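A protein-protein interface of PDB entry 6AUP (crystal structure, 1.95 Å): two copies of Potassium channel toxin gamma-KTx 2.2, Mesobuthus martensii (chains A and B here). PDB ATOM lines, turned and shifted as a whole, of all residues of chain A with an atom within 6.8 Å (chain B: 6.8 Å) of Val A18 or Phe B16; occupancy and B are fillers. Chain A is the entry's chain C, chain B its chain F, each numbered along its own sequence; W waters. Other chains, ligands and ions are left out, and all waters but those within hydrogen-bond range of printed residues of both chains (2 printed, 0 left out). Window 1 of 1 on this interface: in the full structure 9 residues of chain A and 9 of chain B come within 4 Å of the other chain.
The guanidinium group (NH2) of Arg B29 is in salt-bridge range of the side-chain carboxylate (OD1) of Asp A6, 2.8 Å away. The side-chain amide nitrogen (NE2) of Gln A14 is in hydrogen-bond range of the side-chain hydroxyl (OH) of Tyr B13. NE of Arg A22 sits close to ND2 of Asn B27 (3.3 Å).
Water W1 lies within hydrogen-bond range of the side-chain hydroxyl of Ser A21 (2.4 Å), the backbone carbonyl oxygen of Phe B16 (2.7 Å) and the backbone carbonyl oxygen of Lys B25 (2.9 Å). Water W2 lies within hydrogen-bond range of the backbone NH of Val A18 (2.7 Å), the backbone carbonyl oxygen of Gln A14 (2.9 Å) and the backbone carbonyl oxygen of Tyr B13 (3.0 Å).
Of chain B, only Phe B16 comes within 4 Å of Val A18. Phe B16 touches just these residues of chain A: Ile A7 (3.9 Å), Pro A17 (3.9 Å), Val A18 (3.4 Å) and Arg A22 (3.8 Å). Of the printed residues of chain B, Pro A17 touches Phe B16 and Pro B17. Of the printed residues of chain A, Lys B25 touches Ser A21 (3.9 Å). Of the printed residues of chain A, Lys B20 touches Ser A21. Of the printed residues of chain B, Ser A21 touches Lys B20 (3.8 Å), Lys B25 (3.9 Å) and Thr B26 (3.3 Å). Asp A36 touches none of the printed residues of chain B. Cys B35 touches none of the printed residues of chain A. The nearest printed residue of chain A that does not touch Thr B26 is Val A18 (5.5 Å).
Printed residues of chain A that touch a printed residue of chain B: Asp A6, Ile A7, Gln A14, Pro A17, Val A18, Ser A21 and Arg A22. Hydrophobic or aromatic side chains of chain A that line the printed part of chain B: Ile A7, Pro A17 and Val A18. Of the 18 printed residues of chain B, 9 touch a printed residue of chain A. Hydrophobic or aromatic side chains of chain B that line the printed part of chain A: Tyr B13, Phe B16 and Pro B17. Among the printed residues, 15 pairs touch across the chains. Among the printed residues, Asp or Glu carboxylates within 4 Å of a Lys or Arg side-chain nitrogen of the other chain: Asp A6 with Arg B29.
The backbone carbonyl oxygen of Ile A7 sits at hydrogen-bond distance from the backbone NH of Cys A35 (3.0 Å). OG of Ser B21 lies within hydrogen-bond range of O of Pro B17, at 3.3 Å. O of Cys B19 sits at hydrogen-bond distance from N of Lys B25, at 3.2 Å. The side-chain sulfur of Cys A35 is disulfide-bonded to the side-chain sulfur of Cys A15 (2.0 Å). The side-chain sulfur (SG) of Cys B15 is disulfide-bonded to the side-chain sulfur (SG) of Cys B35 (2.0 Å). The side-chain sulfur of Cys B19 is disulfide-bonded to the side-chain sulfur of Cys B37, at 2.0 Å.
Pro A17 touches Phe B16, but with the chains exchanged Phe A16 does not touch Pro B17 (7.2 Å). Pro B17 touches its own counterpart, Pro A17. Val A18 touches Phe B16, but with the chains exchanged Phe A16 does not touch Val B18 (10.7 Å). Ser A21 touches Lys B20, but with the chains exchanged Lys A20 does not touch Ser B21 (10.6 Å). 11 positions are printed for both chains. Of the 15 pairs that touch across the chains among the printed residues, 1 has its exchanged pair printed and touching as well.
Among the printed residues, merely in contact across the chains: Arg A22 with Thr B26 (3.2 Å), Ser A21 with Thr B26 (3.3 Å), Val A18 with Phe B16 (3.4 Å), Ile A7 with Tyr B13 (3.6 Å), Ile A7 with Arg B29 (3.7 Å), Ile A7 with Ser B12 (3.7 Å), Pro A17 with Pro B17 (3.7 Å), Arg A22 with Phe B16 (3.8 Å), Ser A21 with Lys B20 (3.8 Å), Ile A7 with Phe B16 (3.9 Å), Ser A21 with Lys B25 (3.9 Å) and Pro A17 with Phe B16 (3.9 Å).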
ATOM      1  N   THR A   5     -34.336  18.016 -18.957  1.00  0.00           N
ATOM      2  CA  THR A   5     -34.268  18.689 -17.644  1.00  0.00           C
ATOM      3  C   THR A   5     -35.421  19.674 -17.542  1.00  0.00           C
ATOM      4  O   THR A   5     -36.079  20.018 -18.550  1.00  0.00           O
ATOM      5  CB  THR A   5     -32.950  19.480 -17.447  1.00  0.00           C
ATOM      6  OG1 THR A   5     -32.945  20.636 -18.315  1.00  0.00           O
ATOM      7  CG2 THR A   5     -31.736  18.594 -17.739  1.00  0.00           C
ATOM      8  N   ASP A   6     -35.602  20.211 -16.355  1.00  0.00           N
ATOM      9  CA  ASP A   6     -36.543  21.292 -16.167  1.00  0.00           C
ATOM     10  C   ASP A   6     -35.786  22.614 -15.918  1.00  0.00           C
ATOM     11  O   ASP A   6     -36.318  23.548 -15.325  1.00  0.00           O
ATOM     12  CB  ASP A   6     -37.551  20.944 -15.064  1.00  0.00           C
ATOM     13  CG  ASP A   6     -36.901  20.677 -13.714  1.00  0.00           C
ATOM     14  OD1 ASP A   6     -35.685  20.889 -13.549  1.00  0.00           O
ATOM     15  OD2 ASP A   6     -37.634  20.256 -12.790  1.00  0.00           O
ATOM     16  N   ILE A   7     -34.583  22.704 -16.488  1.00  0.00           N
ATOM     17  CA  ILE A   7     -33.671  23.829 -16.258  1.00  0.00           C
ATOM     18  C   ILE A   7     -33.800  24.793 -17.418  1.00  0.00           C
ATOM     19  O   ILE A   7     -33.523  24.435 -18.577  1.00  0.00           O
ATOM     20  CB  ILE A   7     -32.222  23.307 -16.148  1.00  0.00           C
ATOM     21  CG1 ILE A   7     -32.084  22.372 -14.950  1.00  0.00           C
ATOM     22  CG2 ILE A   7     -31.209  24.444 -16.115  1.00  0.00           C
ATOM     23  CD1 ILE A   7     -32.459  22.965 -13.620  1.00  0.00           C
ATOM     24  N   GLN A  14     -25.397  27.225 -21.663  1.00  0.00           N
ATOM     25  CA  GLN A  14     -25.899  27.170 -20.311  1.00  0.00           C
ATOM     26  C   GLN A  14     -26.214  25.747 -19.866  1.00  0.00           C
ATOM     27  O   GLN A  14     -26.282  25.483 -18.687  1.00  0.00           O
ATOM     28  CB  GLN A  14     -27.183  28.035 -20.174  1.00  0.00           C
ATOM     29  CG  GLN A  14     -26.960  29.516 -20.475  1.00  0.00           C
ATOM     30  CD  GLN A  14     -28.230  30.275 -20.789  1.00  0.00           C
ATOM     31  OE1 GLN A  14     -29.278  29.685 -21.128  1.00  0.00           O
ATOM     32  NE2 GLN A  14     -28.147  31.610 -20.699  1.00  0.00           N
ATOM     33  N   CYS A  15     -26.418  24.857 -20.831  1.00  0.00           N
ATOM     34  CA  CYS A  15     -26.789  23.475 -20.573  1.00  0.00           C
ATOM     35  C   CYS A  15     -25.610  22.561 -20.283  1.00  0.00           C
ATOM     36  O   CYS A  15     -25.772  21.478 -19.709  1.00  0.00           O
ATOM     37  CB  CYS A  15     -27.596  22.939 -21.744  1.00  0.00           C
ATOM     38  SG  CYS A  15     -29.139  23.912 -22.013  1.00  0.00           S
ATOM     39  N   PHE A  16     -24.403  22.991 -20.597  1.00  0.00           N
ATOM     40  CA  PHE A  16     -23.287  22.083 -20.448  1.00  0.00           C
ATOM     41  C   PHE A  16     -23.004  21.677 -18.992  1.00  0.00           C
ATOM     42  O   PHE A  16     -22.783  20.482 -18.739  1.00  0.00           O
ATOM     43  CB  PHE A  16     -22.043  22.597 -21.180  1.00  0.00           C
ATOM     44  CG  PHE A  16     -22.114  22.406 -22.655  1.00  0.00           C
ATOM     45  CD1 PHE A  16     -22.880  23.249 -23.429  1.00  0.00           C
ATOM     46  CD2 PHE A  16     -21.483  21.329 -23.269  1.00  0.00           C
ATOM     47  CE1 PHE A  16     -22.960  23.071 -24.799  1.00  0.00           C
ATOM     48  CE2 PHE A  16     -21.556  21.147 -24.624  1.00  0.00           C
ATOM     49  CZ  PHE A  16     -22.288  22.021 -25.401  1.00  0.00           C
ATOM     50  N   PRO A  17     -23.093  22.616 -18.025  1.00  0.00           N
ATOM     51  CA  PRO A  17     -22.898  22.168 -16.628  1.00  0.00           C
ATOM     52  C   PRO A  17     -23.953  21.229 -16.102  1.00  0.00           C
ATOM     53  O   PRO A  17     -23.620  20.288 -15.368  1.00  0.00           O
ATOM     54  CB  PRO A  17     -22.888  23.470 -15.817  1.00  0.00           C
ATOM     55  CG  PRO A  17     -22.665  24.561 -16.811  1.00  0.00           C
ATOM     56  CD  PRO A  17     -23.224  24.085 -18.113  1.00  0.00           C
ATOM     57  N   VAL A  18     -25.227  21.464 -16.411  1.00  0.00           N
ATOM     58  CA  VAL A  18     -26.236  20.546 -15.923  1.00  0.00           C
ATOM     59  C   VAL A  18     -26.082  19.172 -16.566  1.00  0.00           C
ATOM     60  O   VAL A  18     -26.115  18.145 -15.886  1.00  0.00           O
ATOM     61  CB  VAL A  18     -27.674  21.076 -16.073  1.00  0.00           C
ATOM     62  CG1 VAL A  18     -28.027  21.385 -17.512  1.00  0.00           C
ATOM     63  CG2 VAL A  18     -28.644  20.095 -15.464  1.00  0.00           C
ATOM     64  N   CYS A  19     -25.841  19.153 -17.860  1.00  0.00           N
ATOM     65  CA  CYS A  19     -25.739  17.887 -18.563  1.00  0.00           C
ATOM     66  C   CYS A  19     -24.560  17.042 -18.125  1.00  0.00           C
ATOM     67  O   CYS A  19     -24.675  15.798 -18.058  1.00  0.00           O
ATOM     68  CB  CYS A  19     -25.679  18.117 -20.028  1.00  0.00           C
ATOM     69  SG  CYS A  19     -27.226  18.802 -20.623  1.00  0.00           S
ATOM     70  N   LYS A  20     -23.457  17.708 -17.781  1.00  0.00           N
ATOM     71  CA  LYS A  20     -22.279  17.038 -17.247  1.00  0.00           C
ATOM     72  C   LYS A  20     -22.520  16.566 -15.837  1.00  0.00           C
ATOM     73  O   LYS A  20     -22.324  15.387 -15.526  1.00  0.00           O
ATOM     74  CB  LYS A  20     -21.058  17.957 -17.306  1.00  0.00           C
ATOM     75  CG  LYS A  20     -19.741  17.320 -16.825  1.00  0.00           C
ATOM     76  CD  LYS A  20     -19.333  16.074 -17.629  1.00  0.00           C
ATOM     77  CE  LYS A  20     -18.052  15.417 -17.073  1.00  0.00           C
ATOM     78  NZ  LYS A  20     -16.941  16.412 -16.861  1.00  0.00           N
ATOM     79  N   SER A  21     -23.010  17.465 -14.999  1.00  0.00           N
ATOM     80  CA  SER A  21     -23.171  17.187 -13.582  1.00  0.00           C
ATOM     81  C   SER A  21     -24.235  16.091 -13.319  1.00  0.00           C
ATOM     82  O   SER A  21     -23.949  15.095 -12.669  1.00  0.00           O
ATOM     83  CB  SER A  21     -23.502  18.495 -12.833  1.00  0.00           C
ATOM     84  OG  SER A  21     -23.316  18.344 -11.456  1.00  0.00           O
ATOM     85  N   ARG A  22     -25.431  16.257 -13.856  1.00  0.00           N
ATOM     86  CA  ARG A  22     -26.524  15.297 -13.612  1.00  0.00           C
ATOM     87  C   ARG A  22     -26.298  13.935 -14.259  1.00  0.00           C
ATOM     88  O   ARG A  22     -26.734  12.942 -13.725  1.00  0.00           O
ATOM     89  CB  ARG A  22     -27.867  15.829 -14.140  1.00  0.00           C
ATOM     90  CG  ARG A  22     -28.440  17.027 -13.395  1.00  0.00           C
ATOM     91  CD  ARG A  22     -29.270  16.633 -12.189  1.00  0.00           C
ATOM     92  NE  ARG A  22     -30.352  15.669 -12.453  1.00  0.00           N
ATOM     93  CZ  ARG A  22     -31.521  15.942 -13.054  1.00  0.00           C
ATOM     94  NH1 ARG A  22     -31.781  17.153 -13.562  1.00  0.00           N
ATOM     95  NH2 ARG A  22     -32.437  14.975 -13.174  1.00  0.00           N
ATOM     96  N   PHE A  23     -25.740  13.914 -15.466  1.00  0.00           N
ATOM     97  CA  PHE A  23     -25.807  12.728 -16.327  1.00  0.00           C
ATOM     98  C   PHE A  23     -24.456  12.273 -16.880  1.00  0.00           C
ATOM     99  O   PHE A  23     -24.361  11.212 -17.533  1.00  0.00           O
ATOM    100  CB  PHE A  23     -26.749  13.004 -17.505  1.00  0.00           C
ATOM    101  CG  PHE A  23     -28.097  13.465 -17.100  1.00  0.00           C
ATOM    102  CD1 PHE A  23     -28.903  12.667 -16.304  1.00  0.00           C
ATOM    103  CD2 PHE A  23     -28.572  14.706 -17.517  1.00  0.00           C
ATOM    104  CE1 PHE A  23     -30.152  13.100 -15.905  1.00  0.00           C
ATOM    105  CE2 PHE A  23     -29.816  15.147 -17.121  1.00  0.00           C
ATOM    106  CZ  PHE A  23     -30.614  14.340 -16.316  1.00  0.00           C
ATOM    107  N   GLY A  24     -23.415  13.034 -16.595  1.00  0.00           N
ATOM    108  CA  GLY A  24     -22.132  12.845 -17.246  1.00  0.00           C
ATOM    109  C   GLY A  24     -22.203  12.922 -18.754  1.00  0.00           C
ATOM    110  O   GLY A  24     -21.383  12.283 -19.438  1.00  0.00           O
ATOM    111  N   LYS A  25     -23.146  13.716 -19.292  1.00  0.00           N
ATOM    112  CA  LYS A  25     -23.216  13.905 -20.735  1.00  0.00           C
ATOM    113  C   LYS A  25     -22.230  14.980 -21.220  1.00  0.00           C
ATOM    114  O   LYS A  25     -21.849  15.868 -20.492  1.00  0.00           O
ATOM    115  CB  LYS A  25     -24.632  14.252 -21.190  1.00  0.00           C
ATOM    116  CG  LYS A  25     -25.677  13.223 -20.753  1.00  0.00           C
ATOM    117  CD  LYS A  25     -25.601  11.951 -21.567  1.00  0.00           C
ATOM    118  CE  LYS A  25     -26.838  11.090 -21.340  1.00  0.00           C
ATOM    119  NZ  LYS A  25     -26.576   9.715 -21.810  1.00  0.00           N
ATOM    120  N   CYS A  35     -33.115  22.798 -21.007  1.00  0.00           N
ATOM    121  CA  CYS A  35     -31.933  22.034 -21.434  1.00  0.00           C
ATOM    122  C   CYS A  35     -32.277  20.567 -21.768  1.00  0.00           C
ATOM    123  O   CYS A  35     -33.035  19.913 -21.067  1.00  0.00           O
ATOM    124  CB  CYS A  35     -30.820  22.082 -20.372  1.00  0.00           C
ATOM    125  SG  CYS A  35     -30.059  23.724 -20.200  1.00  0.00           S
ATOM    126  N   ASP A  36     -31.711  20.103 -22.864  1.00  0.00           N
ATOM    127  CA  ASP A  36     -31.678  18.682 -23.152  1.00  0.00           C
ATOM    128  C   ASP A  36     -30.234  18.237 -23.209  1.00  0.00           C
ATOM    129  O   ASP A  36     -29.362  19.015 -23.525  1.00  0.00           O
ATOM    130  CB  ASP A  36     -32.391  18.395 -24.456  1.00  0.00           C
ATOM    131  CG  ASP A  36     -33.898  18.322 -24.290  1.00  0.00           C
ATOM    132  OD1 ASP A  36     -34.408  18.412 -23.148  1.00  0.00           O
ATOM    133  OD2 ASP A  36     -34.577  18.147 -25.312  1.00  0.00           O
ATOM    134  N   CYS A  37     -29.989  16.975 -22.829  1.00  0.00           N
ATOM    135  CA  CYS A  37     -28.642  16.441 -22.649  1.00  0.00           C
ATOM    136  C   CYS A  37     -28.433  15.181 -23.477  1.00  0.00           C
ATOM    137  O   CYS A  37     -29.288  14.336 -23.519  1.00  0.00           O
ATOM    138  CB  CYS A  37     -28.377  16.111 -21.180  1.00  0.00           C
ATOM    139  SG  CYS A  37     -28.682  17.481 -20.112  1.00  0.00           S
ATOM    140  N   ALA B  11     -30.638  31.858 -12.179  1.00  0.00           N
ATOM    141  CA  ALA B  11     -31.026  30.730 -13.010  1.00  0.00           C
ATOM    142  C   ALA B  11     -30.427  29.493 -12.416  1.00  0.00           C
ATOM    143  O   ALA B  11     -29.263  29.480 -12.005  1.00  0.00           O
ATOM    144  CB  ALA B  11     -30.524  30.924 -14.424  1.00  0.00           C
ATOM    145  N   SER B  12     -31.204  28.421 -12.382  1.00  0.00           N
ATOM    146  CA  SER B  12     -30.683  27.140 -11.846  1.00  0.00           C
ATOM    147  C   SER B  12     -29.486  26.555 -12.586  1.00  0.00           C
ATOM    148  O   SER B  12     -28.647  25.879 -11.976  1.00  0.00           O
ATOM    149  CB  SER B  12     -31.799  26.107 -11.779  1.00  0.00           C
ATOM    150  OG  SER B  12     -32.705  26.491 -10.788  1.00  0.00           O
ATOM    151  N   TYR B  13     -29.349  26.827 -13.884  1.00  0.00           N
ATOM    152  CA  TYR B  13     -28.175  26.281 -14.603  1.00  0.00           C
ATOM    153  C   TYR B  13     -26.871  26.834 -14.023  1.00  0.00           C
ATOM    154  O   TYR B  13     -25.805  26.232 -14.177  1.00  0.00           O
ATOM    155  CB  TYR B  13     -28.251  26.561 -16.104  1.00  0.00           C
ATOM    156  CG  TYR B  13     -28.118  28.008 -16.503  1.00  0.00           C
ATOM    157  CD1 TYR B  13     -26.882  28.664 -16.465  1.00  0.00           C
ATOM    158  CD2 TYR B  13     -29.238  28.723 -16.993  1.00  0.00           C
ATOM    159  CE1 TYR B  13     -26.771  29.998 -16.843  1.00  0.00           C
ATOM    160  CE2 TYR B  13     -29.133  30.050 -17.376  1.00  0.00           C
ATOM    161  CZ  TYR B  13     -27.915  30.679 -17.306  1.00  0.00           C
ATOM    162  OH  TYR B  13     -27.833  31.985 -17.695  1.00  0.00           O
ATOM    163  N   GLN B  14     -26.944  27.990 -13.372  1.00  0.00           N
ATOM    164  CA  GLN B  14     -25.723  28.651 -12.840  1.00  0.00           C
ATOM    165  C   GLN B  14     -25.189  27.909 -11.621  1.00  0.00           C
ATOM    166  O   GLN B  14     -24.017  28.087 -11.232  1.00  0.00           O
ATOM    167  CB  GLN B  14     -26.035  30.089 -12.459  1.00  0.00           C
ATOM    168  CG  GLN B  14     -26.505  30.954 -13.613  1.00  0.00           C
ATOM    169  CD  GLN B  14     -27.112  32.276 -13.168  1.00  0.00           C
ATOM    170  OE1 GLN B  14     -27.533  32.436 -12.003  1.00  0.00           O
ATOM    171  NE2 GLN B  14     -27.111  33.276 -14.094  1.00  0.00           N
ATOM    172  N   CYS B  15     -26.065  27.093 -11.001  1.00  0.00           N
ATOM    173  CA  CYS B  15     -25.782  26.479  -9.697  1.00  0.00           C
ATOM    174  C   CYS B  15     -25.051  25.132  -9.773  1.00  0.00           C
ATOM    175  O   CYS B  15     -24.410  24.734  -8.808  1.00  0.00           O
ATOM    176  CB  CYS B  15     -27.067  26.338  -8.874  1.00  0.00           C
ATOM    177  SG  CYS B  15     -27.778  27.925  -8.357  1.00  0.00           S
ATOM    178  N   PHE B  16     -25.050  24.480 -10.942  1.00  0.00           N
ATOM    179  CA  PHE B  16     -24.510  23.145 -11.026  1.00  0.00           C
ATOM    180  C   PHE B  16     -22.980  23.122 -10.811  1.00  0.00           C
ATOM    181  O   PHE B  16     -22.475  22.260 -10.092  1.00  0.00           O
ATOM    182  CB  PHE B  16     -24.931  22.462 -12.351  1.00  0.00           C
ATOM    183  CG  PHE B  16     -26.384  22.076 -12.374  1.00  0.00           C
ATOM    184  CD1 PHE B  16     -27.371  23.022 -12.677  1.00  0.00           C
ATOM    185  CD2 PHE B  16     -26.783  20.798 -11.996  1.00  0.00           C
ATOM    186  CE1 PHE B  16     -28.728  22.682 -12.617  1.00  0.00           C
ATOM    187  CE2 PHE B  16     -28.124  20.464 -11.927  1.00  0.00           C
ATOM    188  CZ  PHE B  16     -29.096  21.380 -12.296  1.00  0.00           C
ATOM    189  N   PRO B  17     -22.254  24.096 -11.367  1.00  0.00           N
ATOM    190  CA  PRO B  17     -20.828  24.118 -11.042  1.00  0.00           C
ATOM    191  C   PRO B  17     -20.566  24.390  -9.606  1.00  0.00           C
ATOM    192  O   PRO B  17     -19.698  23.747  -9.030  1.00  0.00           O
ATOM    193  CB  PRO B  17     -20.280  25.262 -11.913  1.00  0.00           C
ATOM    194  CG  PRO B  17     -21.226  25.351 -13.045  1.00  0.00           C
ATOM    195  CD  PRO B  17     -22.576  25.048 -12.448  1.00  0.00           C
ATOM    196  N   VAL B  18     -21.340  25.311  -9.028  1.00  0.00           N
ATOM    197  CA  VAL B  18     -21.283  25.637  -7.597  1.00  0.00           C
ATOM    198  C   VAL B  18     -21.462  24.412  -6.694  1.00  0.00           C
ATOM    199  O   VAL B  18     -20.626  24.118  -5.804  1.00  0.00           O
ATOM    200  CB  VAL B  18     -22.342  26.690  -7.214  1.00  0.00           C
ATOM    201  CG1 VAL B  18     -22.271  26.980  -5.702  1.00  0.00           C
ATOM    202  CG2 VAL B  18     -22.110  27.987  -7.996  1.00  0.00           C
ATOM    203  N   CYS B  19     -22.551  23.709  -6.935  1.00  0.00           N
ATOM    204  CA  CYS B  19     -22.926  22.540  -6.163  1.00  0.00           C
ATOM    205  C   CYS B  19     -21.967  21.399  -6.331  1.00  0.00           C
ATOM    206  O   CYS B  19     -21.694  20.663  -5.371  1.00  0.00           O
ATOM    207  CB  CYS B  19     -24.340  22.107  -6.560  1.00  0.00           C
ATOM    208  SG  CYS B  19     -25.544  23.372  -6.069  1.00  0.00           S
ATOM    209  N   LYS B  20     -21.451  21.215  -7.540  1.00  0.00           N
ATOM    210  CA  LYS B  20     -20.469  20.145  -7.737  1.00  0.00           C
ATOM    211  C   LYS B  20     -19.151  20.440  -7.016  1.00  0.00           C
ATOM    212  O   LYS B  20     -18.590  19.560  -6.355  1.00  0.00           O
ATOM    213  CB  LYS B  20     -20.175  19.893  -9.202  1.00  0.00           C
ATOM    214  CG  LYS B  20     -19.277  18.681  -9.395  1.00  0.00           C
ATOM    215  CD  LYS B  20     -19.629  17.891 -10.631  1.00  0.00           C
ATOM    216  CE  LYS B  20     -19.630  16.401 -10.328  1.00  0.00           C
ATOM    217  NZ  LYS B  20     -19.256  15.649 -11.535  1.00  0.00           N
ATOM    218  N   SER B  21     -18.648  21.663  -7.187  1.00  0.00           N
ATOM    219  CA  SER B  21     -17.381  22.075  -6.579  1.00  0.00           C
ATOM    220  C   SER B  21     -17.450  22.018  -5.084  1.00  0.00           C
ATOM    221  O   SER B  21     -16.595  21.423  -4.449  1.00  0.00           O
ATOM    222  CB  SER B  21     -16.994  23.496  -6.982  1.00  0.00           C
ATOM    223  OG  SER B  21     -16.466  23.497  -8.272  1.00  0.00           O
ATOM    224  N   LYS B  25     -22.110  17.499  -5.126  1.00  0.00           N
ATOM    225  CA  LYS B  25     -23.506  17.236  -5.477  1.00  0.00           C
ATOM    226  C   LYS B  25     -23.813  17.527  -6.938  1.00  0.00           C
ATOM    227  O   LYS B  25     -23.282  18.472  -7.533  1.00  0.00           O
ATOM    228  CB  LYS B  25     -24.424  18.023  -4.587  1.00  0.00           C
ATOM    229  CG  LYS B  25     -24.531  17.431  -3.177  1.00  0.00           C
ATOM    230  CD  LYS B  25     -25.224  18.388  -2.230  1.00  0.00           C
ATOM    231  CE  LYS B  25     -25.273  17.846  -0.787  1.00  0.00           C
ATOM    232  NZ  LYS B  25     -25.904  16.496  -0.748  1.00  0.00           N
ATOM    233  N   THR B  26     -24.674  16.710  -7.516  1.00  0.00           N
ATOM    234  CA  THR B  26     -24.875  16.708  -8.949  1.00  0.00           C
ATOM    235  C   THR B  26     -26.182  17.366  -9.322  1.00  0.00           C
ATOM    236  O   THR B  26     -26.659  17.266 -10.480  1.00  0.00           O
ATOM    237  CB  THR B  26     -24.877  15.278  -9.493  1.00  0.00           C
ATOM    238  OG1 THR B  26     -25.912  14.562  -8.854  1.00  0.00           O
ATOM    239  CG2 THR B  26     -23.532  14.570  -9.227  1.00  0.00           C
ATOM    240  N   ASN B  27     -26.820  17.973  -8.350  1.00  0.00           N
ATOM    241  CA  ASN B  27     -28.047  18.657  -8.600  1.00  0.00           C
ATOM    242  C   ASN B  27     -28.112  19.936  -7.810  1.00  0.00           C
ATOM    243  O   ASN B  27     -27.517  20.050  -6.745  1.00  0.00           O
ATOM    244  CB  ASN B  27     -29.212  17.738  -8.206  1.00  0.00           C
ATOM    245  CG  ASN B  27     -30.358  17.854  -9.134  1.00  0.00           C
ATOM    246  OD1 ASN B  27     -30.625  18.930  -9.648  1.00  0.00           O
ATOM    247  ND2 ASN B  27     -31.023  16.732  -9.408  1.00  0.00           N
ATOM    248  N   GLY B  28     -28.876  20.892  -8.316  1.00  0.00           N
ATOM    249  CA  GLY B  28     -29.212  22.050  -7.539  1.00  0.00           C
ATOM    250  C   GLY B  28     -30.214  22.951  -8.211  1.00  0.00           C
ATOM    251  O   GLY B  28     -30.704  22.660  -9.291  1.00  0.00           O
ATOM    252  N   ARG B  29     -30.454  24.087  -7.588  1.00  0.00           N
ATOM    253  CA  ARG B  29     -31.536  24.944  -7.976  1.00  0.00           C
ATOM    254  C   ARG B  29     -31.302  26.328  -7.380  1.00  0.00           C
ATOM    255  O   ARG B  29     -30.777  26.466  -6.264  1.00  0.00           O
ATOM    256  CB  ARG B  29     -32.855  24.324  -7.502  1.00  0.00           C
ATOM    257  CG  ARG B  29     -34.105  25.191  -7.553  1.00  0.00           C
ATOM    258  CD  ARG B  29     -34.988  25.017  -8.791  1.00  0.00           C
ATOM    259  NE  ARG B  29     -34.914  23.698  -9.401  1.00  0.00           N
ATOM    260  CZ  ARG B  29     -35.223  23.440 -10.678  1.00  0.00           C
ATOM    261  NH1 ARG B  29     -35.680  24.400 -11.500  1.00  0.00           N
ATOM    262  NH2 ARG B  29     -35.085  22.203 -11.141  1.00  0.00           N
ATOM    263  N   CYS B  35     -28.026  29.804  -4.571  1.00  0.00           N
ATOM    264  CA  CYS B  35     -27.895  28.419  -5.015  1.00  0.00           C
ATOM    265  C   CYS B  35     -28.138  27.500  -3.834  1.00  0.00           C
ATOM    266  O   CYS B  35     -27.648  27.742  -2.714  1.00  0.00           O
ATOM    267  CB  CYS B  35     -26.519  28.150  -5.625  1.00  0.00           C
ATOM    268  SG  CYS B  35     -26.298  28.836  -7.280  1.00  0.00           S
ATOM    269  N   CYS B  37     -28.167  23.289  -3.078  1.00  0.00           N
ATOM    270  CA  CYS B  37     -27.608  22.067  -3.656  1.00  0.00           C
ATOM    271  C   CYS B  37     -28.234  20.804  -3.064  1.00  0.00           C
ATOM    272  O   CYS B  37     -28.364  20.708  -1.856  1.00  0.00           O
ATOM    273  CB  CYS B  37     -26.109  22.037  -3.432  1.00  0.00           C
ATOM    274  SG  CYS B  37     -25.282  23.492  -4.082  1.00  0.00           S
HETATM  275  O   HOH W   1     -24.026  20.006  -9.833  1.00  0.00           O
HETATM  276  O   HOH W   2     -26.203  24.019 -16.139  1.00  0.00           O
